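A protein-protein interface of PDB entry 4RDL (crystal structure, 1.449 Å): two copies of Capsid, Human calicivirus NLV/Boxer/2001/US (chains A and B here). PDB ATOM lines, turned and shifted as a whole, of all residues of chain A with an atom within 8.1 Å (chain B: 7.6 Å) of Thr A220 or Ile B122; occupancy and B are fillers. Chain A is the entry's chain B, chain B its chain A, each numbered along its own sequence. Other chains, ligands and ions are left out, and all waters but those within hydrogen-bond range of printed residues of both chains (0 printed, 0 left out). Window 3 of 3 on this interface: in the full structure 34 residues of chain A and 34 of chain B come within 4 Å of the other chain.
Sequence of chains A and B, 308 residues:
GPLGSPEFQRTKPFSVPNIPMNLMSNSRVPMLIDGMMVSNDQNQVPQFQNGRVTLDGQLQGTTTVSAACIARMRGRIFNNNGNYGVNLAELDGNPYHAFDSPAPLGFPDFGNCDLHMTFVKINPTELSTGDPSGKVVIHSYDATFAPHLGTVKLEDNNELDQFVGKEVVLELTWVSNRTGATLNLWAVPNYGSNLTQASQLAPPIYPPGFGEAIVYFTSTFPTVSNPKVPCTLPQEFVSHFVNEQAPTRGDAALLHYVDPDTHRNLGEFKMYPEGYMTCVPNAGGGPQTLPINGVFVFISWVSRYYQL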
ATOM      1  N   ASN A  26     -22.886  16.547  -4.712  1.00  0.00           N
ATOM      2  CA  ASN A  26     -23.900  17.573  -4.900  1.00  0.00           C
ATOM      3  C   ASN A  26     -23.298  18.929  -4.484  1.00  0.00           C
ATOM      4  O   ASN A  26     -22.402  18.980  -3.621  1.00  0.00           O
ATOM      5  CB  ASN A  26     -25.103  17.232  -4.013  1.00  0.00           C
ATOM      6  CG  ASN A  26     -26.406  17.849  -4.498  1.00  0.00           C
ATOM      7  OD1 ASN A  26     -26.642  19.043  -4.321  1.00  0.00           O
ATOM      8  ND2 ASN A  26     -27.282  17.019  -5.073  1.00  0.00           N
ATOM      9  N   VAL A  29     -25.828  20.002  -0.984  1.00  0.00           N
ATOM     10  CA  VAL A  29     -25.576  19.231   0.234  1.00  0.00           C
ATOM     11  C   VAL A  29     -24.316  18.429  -0.021  1.00  0.00           C
ATOM     12  O   VAL A  29     -24.029  18.085  -1.165  1.00  0.00           O
ATOM     13  CB  VAL A  29     -26.740  18.247   0.598  1.00  0.00           C
ATOM     14  CG1 VAL A  29     -27.980  19.014   1.056  1.00  0.00           C
ATOM     15  CG2 VAL A  29     -27.074  17.331  -0.579  1.00  0.00           C
ATOM     16  N   PRO A  30     -23.540  18.145   1.037  1.00  0.00           N
ATOM     17  CA  PRO A  30     -22.322  17.341   0.872  1.00  0.00           C
ATOM     18  C   PRO A  30     -22.685  15.858   0.832  1.00  0.00           C
ATOM     19  O   PRO A  30     -22.657  15.146   1.842  1.00  0.00           O
ATOM     20  CB  PRO A  30     -21.508  17.695   2.120  1.00  0.00           C
ATOM     21  CG  PRO A  30     -22.559  17.993   3.155  1.00  0.00           C
ATOM     22  CD  PRO A  30     -23.673  18.683   2.404  1.00  0.00           C
ATOM     23  N   MET A  31     -23.051  15.414  -0.362  1.00  0.00           N
ATOM     24  CA  MET A  31     -23.541  14.067  -0.590  1.00  0.00           C
ATOM     25  C   MET A  31     -23.155  13.682  -2.006  1.00  0.00           C
ATOM     26  O   MET A  31     -23.274  14.501  -2.919  1.00  0.00           O
ATOM     27  CB  MET A  31     -25.064  14.055  -0.494  1.00  0.00           C
ATOM     28  CG  MET A  31     -25.632  12.846   0.170  1.00  0.00           C
ATOM     29  SD  MET A  31     -25.210  12.827   1.918  1.00  0.00           S
ATOM     30  CE  MET A  31     -26.486  11.735   2.500  1.00  0.00           C
ATOM     31  N   LEU A  32     -22.714  12.443  -2.207  1.00  0.00           N
ATOM     32  CA  LEU A  32     -22.399  11.989  -3.554  1.00  0.00           C
ATOM     33  C   LEU A  32     -23.613  12.116  -4.466  1.00  0.00           C
ATOM     34  O   LEU A  32     -24.773  11.925  -4.039  1.00  0.00           O
ATOM     35  CB  LEU A  32     -21.917  10.540  -3.544  1.00  0.00           C
ATOM     36  CG  LEU A  32     -20.555  10.283  -2.900  1.00  0.00           C
ATOM     37  CD1 LEU A  32     -20.308   8.775  -2.732  1.00  0.00           C
ATOM     38  CD2 LEU A  32     -19.434  10.948  -3.685  1.00  0.00           C
ATOM     39  N   ILE A  33     -23.342  12.430  -5.728  1.00  0.00           N
ATOM     40  CA  ILE A  33     -24.371  12.407  -6.759  1.00  0.00           C
ATOM     41  C   ILE A  33     -24.773  10.965  -7.070  1.00  0.00           C
ATOM     42  O   ILE A  33     -23.917  10.107  -7.291  1.00  0.00           O
ATOM     43  CB  ILE A  33     -23.881  13.108  -8.048  1.00  0.00           C
ATOM     44  CG1 ILE A  33     -23.644  14.600  -7.774  1.00  0.00           C
ATOM     45  CG2 ILE A  33     -24.881  12.924  -9.191  1.00  0.00           C
ATOM     46  CD1 ILE A  33     -22.899  15.298  -8.868  1.00  0.00           C
ATOM     47  N   ASP A  34     -26.076  10.697  -7.085  1.00  0.00           N
ATOM     48  CA  ASP A  34     -26.553   9.353  -7.407  1.00  0.00           C
ATOM     49  C   ASP A  34     -27.574   9.343  -8.539  1.00  0.00           C
ATOM     50  O   ASP A  34     -28.272   8.350  -8.753  1.00  0.00           O
ATOM     51  CB  ASP A  34     -27.091   8.640  -6.162  1.00  0.00           C
ATOM     52  CG  ASP A  34     -28.368   9.247  -5.636  1.00  0.00           C
ATOM     53  OD1 ASP A  34     -28.790  10.304  -6.137  1.00  0.00           O
ATOM     54  OD2 ASP A  34     -28.971   8.641  -4.724  1.00  0.00           O
ATOM     55  N   GLY A  35     -27.659  10.442  -9.277  1.00  0.00           N
ATOM     56  CA  GLY A  35     -28.538  10.482 -10.431  1.00  0.00           C
ATOM     57  C   GLY A  35     -28.531  11.805 -11.167  1.00  0.00           C
ATOM     58  O   GLY A  35     -27.909  12.781 -10.726  1.00  0.00           O
ATOM     59  N   PHE A 217     -28.374  17.402 -11.198  1.00  0.00           N
ATOM     60  CA  PHE A 217     -27.659  16.337 -10.536  1.00  0.00           C
ATOM     61  C   PHE A 217     -28.289  16.135  -9.167  1.00  0.00           C
ATOM     62  O   PHE A 217     -28.502  17.095  -8.422  1.00  0.00           O
ATOM     63  CB  PHE A 217     -26.181  16.720 -10.453  1.00  0.00           C
ATOM     64  CG  PHE A 217     -25.600  17.043 -11.797  1.00  0.00           C
ATOM     65  CD1 PHE A 217     -25.116  16.034 -12.610  1.00  0.00           C
ATOM     66  CD2 PHE A 217     -25.602  18.352 -12.276  1.00  0.00           C
ATOM     67  CE1 PHE A 217     -24.620  16.321 -13.865  1.00  0.00           C
ATOM     68  CE2 PHE A 217     -25.104  18.648 -13.530  1.00  0.00           C
ATOM     69  CZ  PHE A 217     -24.614  17.630 -14.328  1.00  0.00           C
ATOM     70  N   THR A 218     -28.620  14.891  -8.845  1.00  0.00           N
ATOM     71  CA  THR A 218     -29.400  14.612  -7.645  1.00  0.00           C
ATOM     72  C   THR A 218     -28.627  13.790  -6.633  1.00  0.00           C
ATOM     73  O   THR A 218     -27.737  13.010  -6.999  1.00  0.00           O
ATOM     74  CB  THR A 218     -30.727  13.896  -7.973  1.00  0.00           C
ATOM     75  OG1 THR A 218     -30.456  12.613  -8.554  1.00  0.00           O
ATOM     76  CG2 THR A 218     -31.540  14.734  -8.949  1.00  0.00           C
ATOM     77  N   SER A 219     -28.989  13.964  -5.362  1.00  0.00           N
ATOM     78  CA  SER A 219     -28.498  13.124  -4.277  1.00  0.00           C
ATOM     79  C   SER A 219     -29.663  12.738  -3.379  1.00  0.00           C
ATOM     80  O   SER A 219     -30.507  13.568  -3.035  1.00  0.00           O
ATOM     81  CB  SER A 219     -27.472  13.877  -3.422  1.00  0.00           C
ATOM     82  OG  SER A 219     -26.347  14.254  -4.189  1.00  0.00           O
ATOM     83  N   THR A 220     -29.694  11.480  -2.968  1.00  0.00           N
ATOM     84  CA  THR A 220     -30.601  11.079  -1.915  1.00  0.00           C
ATOM     85  C   THR A 220     -30.120  11.702  -0.601  1.00  0.00           C
ATOM     86  O   THR A 220     -28.944  11.598  -0.241  1.00  0.00           O
ATOM     87  CB  THR A 220     -30.686   9.554  -1.816  1.00  0.00           C
ATOM     88  OG1 THR A 220     -31.140   9.041  -3.071  1.00  0.00           O
ATOM     89  CG2 THR A 220     -31.646   9.139  -0.713  1.00  0.00           C
ATOM     90  N   PHE A 221     -31.033  12.358   0.107  1.00  0.00           N
ATOM     91  CA  PHE A 221     -30.681  13.140   1.284  1.00  0.00           C
ATOM     92  C   PHE A 221     -31.943  13.273   2.120  1.00  0.00           C
ATOM     93  O   PHE A 221     -33.043  13.243   1.573  1.00  0.00           O
ATOM     94  CB  PHE A 221     -30.183  14.522   0.829  1.00  0.00           C
ATOM     95  CG  PHE A 221     -29.785  15.439   1.957  1.00  0.00           C
ATOM     96  CD1 PHE A 221     -28.482  15.446   2.438  1.00  0.00           C
ATOM     97  CD2 PHE A 221     -30.707  16.306   2.525  1.00  0.00           C
ATOM     98  CE1 PHE A 221     -28.117  16.288   3.475  1.00  0.00           C
ATOM     99  CE2 PHE A 221     -30.345  17.138   3.565  1.00  0.00           C
ATOM    100  CZ  PHE A 221     -29.051  17.132   4.037  1.00  0.00           C
ATOM    101  N   PRO A 222     -31.798  13.415   3.445  1.00  0.00           N
ATOM    102  CA  PRO A 222     -32.975  13.524   4.313  1.00  0.00           C
ATOM    103  C   PRO A 222     -33.656  14.898   4.282  1.00  0.00           C
ATOM    104  O   PRO A 222     -33.802  15.564   5.314  1.00  0.00           O
ATOM    105  CB  PRO A 222     -32.414  13.206   5.699  1.00  0.00           C
ATOM    106  CG  PRO A 222     -30.981  13.686   5.617  1.00  0.00           C
ATOM    107  CD  PRO A 222     -30.554  13.275   4.226  1.00  0.00           C
ATOM    108  N   THR A 223     -34.055  15.318   3.085  1.00  0.00           N
ATOM    109  CA  THR A 223     -35.075  16.347   2.928  1.00  0.00           C
ATOM    110  C   THR A 223     -36.398  15.596   3.046  1.00  0.00           C
ATOM    111  O   THR A 223     -36.928  15.057   2.071  1.00  0.00           O
ATOM    112  CB  THR A 223     -34.944  17.088   1.576  1.00  0.00           C
ATOM    113  OG1 THR A 223     -34.409  16.193   0.592  1.00  0.00           O
ATOM    114  CG2 THR A 223     -34.006  18.295   1.708  1.00  0.00           C
ATOM    115  N   ASN A 226     -39.394  14.753   0.615  1.00  0.00           N
ATOM    116  CA  ASN A 226     -38.887  14.997  -0.725  1.00  0.00           C
ATOM    117  C   ASN A 226     -37.383  14.712  -0.769  1.00  0.00           C
ATOM    118  O   ASN A 226     -36.576  15.628  -0.958  1.00  0.00           O
ATOM    119  CB  ASN A 226     -39.191  16.444  -1.108  1.00  0.00           C
ATOM    120  CG  ASN A 226     -38.945  16.733  -2.560  1.00  0.00           C
ATOM    121  OD1 ASN A 226     -38.614  15.840  -3.344  1.00  0.00           O
ATOM    122  ND2 ASN A 226     -39.127  17.991  -2.938  1.00  0.00           N
ATOM    123  N   PRO A 227     -37.005  13.433  -0.584  1.00  0.00           N
ATOM    124  CA  PRO A 227     -35.618  13.074  -0.248  1.00  0.00           C
ATOM    125  C   PRO A 227     -34.679  12.950  -1.445  1.00  0.00           C
ATOM    126  O   PRO A 227     -33.872  12.016  -1.519  1.00  0.00           O
ATOM    127  CB  PRO A 227     -35.777  11.722   0.449  1.00  0.00           C
ATOM    128  CG  PRO A 227     -36.987  11.112  -0.215  1.00  0.00           C
ATOM    129  CD  PRO A 227     -37.915  12.274  -0.490  1.00  0.00           C
ATOM    130  N   LYS A 228     -34.782  13.895  -2.369  1.00  0.00           N
ATOM    131  CA  LYS A 228     -33.920  13.935  -3.541  1.00  0.00           C
ATOM    132  C   LYS A 228     -33.563  15.383  -3.822  1.00  0.00           C
ATOM    133  O   LYS A 228     -34.413  16.169  -4.249  1.00  0.00           O
ATOM    134  CB  LYS A 228     -34.617  13.323  -4.761  1.00  0.00           C
ATOM    135  CG  LYS A 228     -33.730  13.314  -5.988  1.00  0.00           C
ATOM    136  CD  LYS A 228     -34.209  12.344  -7.048  1.00  0.00           C
ATOM    137  CE  LYS A 228     -35.416  12.873  -7.789  1.00  0.00           C
ATOM    138  NZ  LYS A 228     -35.810  11.937  -8.877  1.00  0.00           N
ATOM    139  N   VAL A 229     -32.308  15.739  -3.566  1.00  0.00           N
ATOM    140  CA  VAL A 229     -31.880  17.134  -3.684  1.00  0.00           C
ATOM    141  C   VAL A 229     -31.282  17.397  -5.062  1.00  0.00           C
ATOM    142  O   VAL A 229     -30.290  16.777  -5.433  1.00  0.00           O
ATOM    143  CB  VAL A 229     -30.836  17.503  -2.610  1.00  0.00           C
ATOM    144  CG1 VAL A 229     -30.236  18.881  -2.901  1.00  0.00           C
ATOM    145  CG2 VAL A 229     -31.457  17.452  -1.215  1.00  0.00           C
ATOM    146  N   PRO A 230     -31.897  18.301  -5.836  1.00  0.00           N
ATOM    147  CA  PRO A 230     -31.373  18.652  -7.160  1.00  0.00           C
ATOM    148  C   PRO A 230     -30.388  19.817  -7.103  1.00  0.00           C
ATOM    149  O   PRO A 230     -30.565  20.730  -6.293  1.00  0.00           O
ATOM    150  CB  PRO A 230     -32.631  19.079  -7.906  1.00  0.00           C
ATOM    151  CG  PRO A 230     -33.461  19.748  -6.829  1.00  0.00           C
ATOM    152  CD  PRO A 230     -33.158  19.006  -5.540  1.00  0.00           C
ATOM    153  N   ARG B  74     -21.426   4.423   6.310  1.00  0.00           N
ATOM    154  CA  ARG B  74     -22.761   4.029   5.888  1.00  0.00           C
ATOM    155  C   ARG B  74     -22.969   2.567   6.226  1.00  0.00           C
ATOM    156  O   ARG B  74     -22.045   1.762   6.134  1.00  0.00           O
ATOM    157  CB  ARG B  74     -22.954   4.248   4.384  1.00  0.00           C
ATOM    158  CG  ARG B  74     -24.339   3.843   3.876  1.00  0.00           C
ATOM    159  CD  ARG B  74     -24.587   4.369   2.468  1.00  0.00           C
ATOM    160  NE  ARG B  74     -25.888   3.941   1.957  1.00  0.00           N
ATOM    161  CZ  ARG B  74     -26.554   4.556   0.989  1.00  0.00           C
ATOM    162  NH1 ARG B  74     -26.041   5.640   0.417  1.00  0.00           N
ATOM    163  NH2 ARG B  74     -27.736   4.088   0.598  1.00  0.00           N
ATOM    164  N   GLY B  75     -24.187   2.217   6.611  1.00  0.00           N
ATOM    165  CA  GLY B  75     -24.524   0.810   6.726  1.00  0.00           C
ATOM    166  C   GLY B  75     -25.820   0.574   7.455  1.00  0.00           C
ATOM    167  O   GLY B  75     -26.583   1.505   7.722  1.00  0.00           O
ATOM    168  N   LEU B  91     -20.167   4.532   0.892  1.00  0.00           N
ATOM    169  CA  LEU B  91     -21.060   5.665   1.133  1.00  0.00           C
ATOM    170  C   LEU B  91     -22.181   5.808   0.097  1.00  0.00           C
ATOM    171  O   LEU B  91     -23.211   6.415   0.376  1.00  0.00           O
ATOM    172  CB  LEU B  91     -20.259   6.960   1.243  1.00  0.00           C
ATOM    173  CG  LEU B  91     -19.348   7.028   2.472  1.00  0.00           C
ATOM    174  CD1 LEU B  91     -18.480   8.296   2.423  1.00  0.00           C
ATOM    175  CD2 LEU B  91     -20.152   6.988   3.748  1.00  0.00           C
ATOM    176  N   GLY B  93     -23.842   3.306  -0.954  1.00  0.00           N
ATOM    177  CA  GLY B  93     -24.757   2.208  -0.688  1.00  0.00           C
ATOM    178  C   GLY B  93     -24.371   0.894  -1.352  1.00  0.00           C
ATOM    179  O   GLY B  93     -24.947  -0.147  -1.054  1.00  0.00           O
ATOM    180  N   PHE B 119     -26.176  10.667  12.756  1.00  0.00           N
ATOM    181  CA  PHE B 119     -26.614   9.866  11.623  1.00  0.00           C
ATOM    182  C   PHE B 119     -28.045  10.144  11.200  1.00  0.00           C
ATOM    183  O   PHE B 119     -28.849  10.683  11.969  1.00  0.00           O
ATOM    184  CB  PHE B 119     -26.407   8.363  11.870  1.00  0.00           C
ATOM    185  CG  PHE B 119     -27.276   7.785  12.960  1.00  0.00           C
ATOM    186  CD1 PHE B 119     -28.584   7.385  12.696  1.00  0.00           C
ATOM    187  CD2 PHE B 119     -26.779   7.620  14.244  1.00  0.00           C
ATOM    188  CE1 PHE B 119     -29.372   6.844  13.696  1.00  0.00           C
ATOM    189  CE2 PHE B 119     -27.560   7.070  15.244  1.00  0.00           C
ATOM    190  CZ  PHE B 119     -28.855   6.687  14.970  1.00  0.00           C
ATOM    191  N   VAL B 120     -28.349   9.764   9.962  1.00  0.00           N
ATOM    192  CA  VAL B 120     -29.701   9.852   9.433  1.00  0.00           C
ATOM    193  C   VAL B 120     -30.034   8.591   8.648  1.00  0.00           C
ATOM    194  O   VAL B 120     -29.166   8.009   7.986  1.00  0.00           O
ATOM    195  CB  VAL B 120     -29.870  11.081   8.505  1.00  0.00           C
ATOM    196  CG1 VAL B 120     -29.738  12.388   9.304  1.00  0.00           C
ATOM    197  CG2 VAL B 120     -28.884  11.050   7.337  1.00  0.00           C
ATOM    198  N   LYS B 121     -31.293   8.169   8.718  1.00  0.00           N
ATOM    199  CA  LYS B 121     -31.772   7.139   7.806  1.00  0.00           C
ATOM    200  C   LYS B 121     -31.613   7.632   6.370  1.00  0.00           C
ATOM    201  O   LYS B 121     -31.774   8.829   6.099  1.00  0.00           O
ATOM    202  CB  LYS B 121     -33.239   6.809   8.105  1.00  0.00           C
ATOM    203  CG  LYS B 121     -33.438   6.158   9.463  1.00  0.00           C
ATOM    204  CD  LYS B 121     -34.851   5.587   9.623  1.00  0.00           C
ATOM    205  CE  LYS B 121     -35.898   6.686   9.601  1.00  0.00           C
ATOM    206  NZ  LYS B 121     -37.268   6.131   9.908  1.00  0.00           N
ATOM    207  N   ILE B 122     -31.272   6.727   5.456  1.00  0.00           N
ATOM    208  CA  ILE B 122     -30.950   7.132   4.085  1.00  0.00           C
ATOM    209  C   ILE B 122     -31.803   6.441   3.005  1.00  0.00           C
ATOM    210  O   ILE B 122     -31.727   6.796   1.840  1.00  0.00           O
ATOM    211  CB  ILE B 122     -29.421   6.981   3.809  1.00  0.00           C
ATOM    212  CG1 ILE B 122     -28.975   7.820   2.601  1.00  0.00           C
ATOM    213  CG2 ILE B 122     -29.021   5.515   3.690  1.00  0.00           C
ATOM    214  CD1 ILE B 122     -29.237   9.306   2.761  1.00  0.00           C
ATOM    215  N   ASN B 123     -32.611   5.460   3.395  1.00  0.00           N
ATOM    216  CA  ASN B 123     -33.565   4.861   2.465  1.00  0.00           C
ATOM    217  C   ASN B 123     -34.706   5.846   2.206  1.00  0.00           C
ATOM    218  O   ASN B 123     -35.359   6.299   3.145  1.00  0.00           O
ATOM    219  CB  ASN B 123     -34.106   3.552   3.053  1.00  0.00           C
ATOM    220  CG  ASN B 123     -34.945   2.752   2.067  1.00  0.00           C
ATOM    221  OD1 ASN B 123     -35.534   3.291   1.139  1.00  0.00           O
ATOM    222  ND2 ASN B 123     -35.018   1.448   2.295  1.00  0.00           N
ATOM    223  N   PRO B 124     -34.960   6.180   0.932  1.00  0.00           N
ATOM    224  CA  PRO B 124     -36.029   7.148   0.650  1.00  0.00           C
ATOM    225  C   PRO B 124     -37.381   6.760   1.258  1.00  0.00           C
ATOM    226  O   PRO B 124     -38.155   7.650   1.616  1.00  0.00           O
ATOM    227  CB  PRO B 124     -36.111   7.160  -0.881  1.00  0.00           C
ATOM    228  CG  PRO B 124     -34.795   6.694  -1.338  1.00  0.00           C
ATOM    229  CD  PRO B 124     -34.222   5.789  -0.282  1.00  0.00           C
ATOM    230  N   THR B 125     -37.672   5.467   1.384  1.00  0.00           N
ATOM    231  CA  THR B 125     -38.956   5.061   1.951  1.00  0.00           C
ATOM    232  C   THR B 125     -39.046   5.363   3.445  1.00  0.00           C
ATOM    233  O   THR B 125     -40.135   5.338   4.028  1.00  0.00           O
ATOM    234  CB  THR B 125     -39.247   3.567   1.710  1.00  0.00           C
ATOM    235  OG1 THR B 125     -38.292   2.765   2.421  1.00  0.00           O
ATOM    236  CG2 THR B 125     -39.170   3.248   0.232  1.00  0.00           C
ATOM    237  N   GLU B 126     -37.897   5.645   4.058  1.00  0.00           N
ATOM    238  CA  GLU B 126     -37.827   5.991   5.475  1.00  0.00           C
ATOM    239  C   GLU B 126     -37.761   7.502   5.662  1.00  0.00           C
ATOM    240  O   GLU B 126     -37.589   7.993   6.780  1.00  0.00           O
ATOM    241  CB  GLU B 126     -36.603   5.341   6.127  1.00  0.00           C
ATOM    242  CG  GLU B 126     -36.655   3.824   6.157  1.00  0.00           C
ATOM    243  CD  GLU B 126     -37.617   3.289   7.193  1.00  0.00           C
ATOM    244  OE1 GLU B 126     -37.940   4.029   8.150  1.00  0.00           O
ATOM    245  OE2 GLU B 126     -38.046   2.124   7.050  1.00  0.00           O
ATOM    246  N   LEU B 127     -37.901   8.232   4.562  1.00  0.00           N
ATOM    247  CA  LEU B 127     -37.727   9.684   4.572  1.00  0.00           C
ATOM    248  C   LEU B 127     -38.960  10.439   4.056  1.00  0.00           C
ATOM    249  O   LEU B 127     -38.837  11.525   3.478  1.00  0.00           O
ATOM    250  CB  LEU B 127     -36.479  10.076   3.761  1.00  0.00           C
ATOM    251  CG  LEU B 127     -35.139   9.578   4.312  1.00  0.00           C
ATOM    252  CD1 LEU B 127     -33.989   9.824   3.331  1.00  0.00           C
ATOM    253  CD2 LEU B 127     -34.838  10.201   5.678  1.00  0.00           C
ATOM    254  N   PRO B 132     -35.581  11.590  10.985  1.00  0.00           N
ATOM    255  CA  PRO B 132     -34.780  10.437  10.562  1.00  0.00           C
ATOM    256  C   PRO B 132     -33.440  10.356  11.281  1.00  0.00           C
ATOM    257  O   PRO B 132     -32.630   9.488  10.944  1.00  0.00           O
ATOM    258  CB  PRO B 132     -34.524  10.743   9.093  1.00  0.00           C
ATOM    259  CG  PRO B 132     -34.359  12.248   9.080  1.00  0.00           C
ATOM    260  CD  PRO B 132     -35.351  12.763  10.122  1.00  0.00           C
ATOM    261  N   LYS B 166     -32.401  -0.621   9.834  1.00  0.00           N
ATOM    262  CA  LYS B 166     -32.448   0.519   8.921  1.00  0.00           C
ATOM    263  C   LYS B 166     -31.059   0.908   8.427  1.00  0.00           C
ATOM    264  O   LYS B 166     -30.082   0.829   9.173  1.00  0.00           O
ATOM    265  CB  LYS B 166     -33.067   1.745   9.597  1.00  0.00           C
ATOM    266  CG  LYS B 166     -34.381   1.497  10.314  1.00  0.00           C
ATOM    267  CD  LYS B 166     -35.485   1.139   9.365  1.00  0.00           C
ATOM    268  CE  LYS B 166     -36.834   1.176  10.092  1.00  0.00           C
ATOM    269  NZ  LYS B 166     -37.926   0.578   9.288  1.00  0.00           N
ATOM    270  N   GLU B 167     -30.987   1.340   7.172  1.00  0.00           N
ATOM    271  CA  GLU B 167     -29.739   1.845   6.616  1.00  0.00           C
ATOM    272  C   GLU B 167     -29.568   3.314   6.963  1.00  0.00           C
ATOM    273  O   GLU B 167     -30.489   4.120   6.809  1.00  0.00           O
ATOM    274  CB  GLU B 167     -29.678   1.668   5.100  1.00  0.00           C
ATOM    275  CG  GLU B 167     -28.258   1.790   4.567  1.00  0.00           C
ATOM    276  CD  GLU B 167     -28.166   1.777   3.061  1.00  0.00           C
ATOM    277  OE1 GLU B 167     -29.186   2.030   2.394  1.00  0.00           O
ATOM    278  OE2 GLU B 167     -27.055   1.522   2.543  1.00  0.00           O
ATOM    279  N   VAL B 168     -28.380   3.648   7.450  1.00  0.00           N
ATOM    280  CA  VAL B 168     -28.079   5.026   7.834  1.00  0.00           C
ATOM    281  C   VAL B 168     -26.761   5.488   7.232  1.00  0.00           C
ATOM    282  O   VAL B 168     -25.909   4.674   6.874  1.00  0.00           O
ATOM    283  CB  VAL B 168     -28.021   5.197   9.383  1.00  0.00           C
ATOM    284  CG1 VAL B 168     -29.351   4.799  10.033  1.00  0.00           C
ATOM    285  CG2 VAL B 168     -26.853   4.407   9.996  1.00  0.00           C
ATOM    286  N   VAL B 169     -26.615   6.804   7.108  1.00  0.00           N
ATOM    287  CA  VAL B 169     -25.311   7.406   6.878  1.00  0.00           C
ATOM    288  C   VAL B 169     -24.901   8.153   8.140  1.00  0.00           C
ATOM    289  O   VAL B 169     -25.729   8.816   8.790  1.00  0.00           O
ATOM    290  CB  VAL B 169     -25.303   8.324   5.640  1.00  0.00           C
ATOM    291  CG1 VAL B 169     -25.431   7.500   4.373  1.00  0.00           C
ATOM    292  CG2 VAL B 169     -26.395   9.355   5.710  1.00  0.00           C
ATOM    293  N   LEU B 170     -23.635   7.996   8.512  1.00  0.00           N
ATOM    294  CA  LEU B 170     -23.107   8.574   9.741  1.00  0.00           C
ATOM    295  C   LEU B 170     -22.013   9.568   9.402  1.00  0.00           C
ATOM    296  O   LEU B 170     -21.248   9.369   8.455  1.00  0.00           O
ATOM    297  CB  LEU B 170     -22.545   7.479  10.647  1.00  0.00           C
ATOM    298  CG  LEU B 170     -23.491   6.318  10.995  1.00  0.00           C
ATOM    299  CD1 LEU B 170     -23.144   5.080  10.169  1.00  0.00           C
ATOM    300  CD2 LEU B 170     -23.392   6.012  12.472  1.00  0.00           C
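Of the 19 printed residues of chain B, 4 touch a printed residue of chain A. Printed residues of chain B that touch a printed residue of chain A: Val B120, Ile B122, Leu B127 and Val B169. Hydrophobic or aromatic side chains of chain B within 4 Å of the printed part of chain A: Val B120, Ile B122, Leu B127 and Val B169. Among the printed residues, 7 pairs touch across the chains. Among the printed residues, no Asp or Glu carboxylate lies within 4 Å of a Lys or Arg side-chain nitrogen of the other chain.
CE of Met A31 touches CD1 of Ile B122 (3.7 Å). CE of Met A31 touches CG2 of Val B169, at 3.997 Å. Ile B122 touches Thr A220 (O to CG2, 3.5 Å). Phe A221 touches Leu B127 (O to CD1, 3.96 Å). CG2 of Val B120 touches CG of Pro A222, 3.8 Å away. Pro A222 touches Leu B127 (CB to CD2, 3.9 Å). CB of Pro A227 touches CB of Leu B127, 3.8 Å away.
The backbone NH (N) of Val B169 lies within hydrogen-bond range of the backbone carbonyl oxygen (O) of Val B120 (3.0 Å). O of Glu B167 is in hydrogen-bond range of N of Ile B122, 3.0 Å away. N of Asn A26 sits at hydrogen-bond distance from O of Met A31. The backbone carbonyl oxygen of Phe A221 is in hydrogen-bond range of the side-chain hydroxyl of Thr A223. OD2 of Asp A34 sits at hydrogen-bond distance from OG1 of Thr A220 (2.8 Å). The backbone carbonyl oxygen of Pro A227 sits at hydrogen-bond distance from the backbone NH of Phe A221, at 3.3 Å.
No position is printed for both chains.
Of the printed residues of chain B, Met A31 touches Ile B122 and Val B169. Thr A220 touches one residue of chain B. Of the printed residues of chain B, Pro A227 touches Leu B127. Of the printed residues of chain A, Val B120 touches Pro A222 (3.8 Å). Of chain A, only Met A31 and Thr A220 come within 4 Å of Ile B122. The nearest residue of chain B that does not touch Thr A220 is Pro B124 (4.04 Å). The nearest printed residue of chain A that does not touch Val B120 is Met A31 (5.4 Å).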
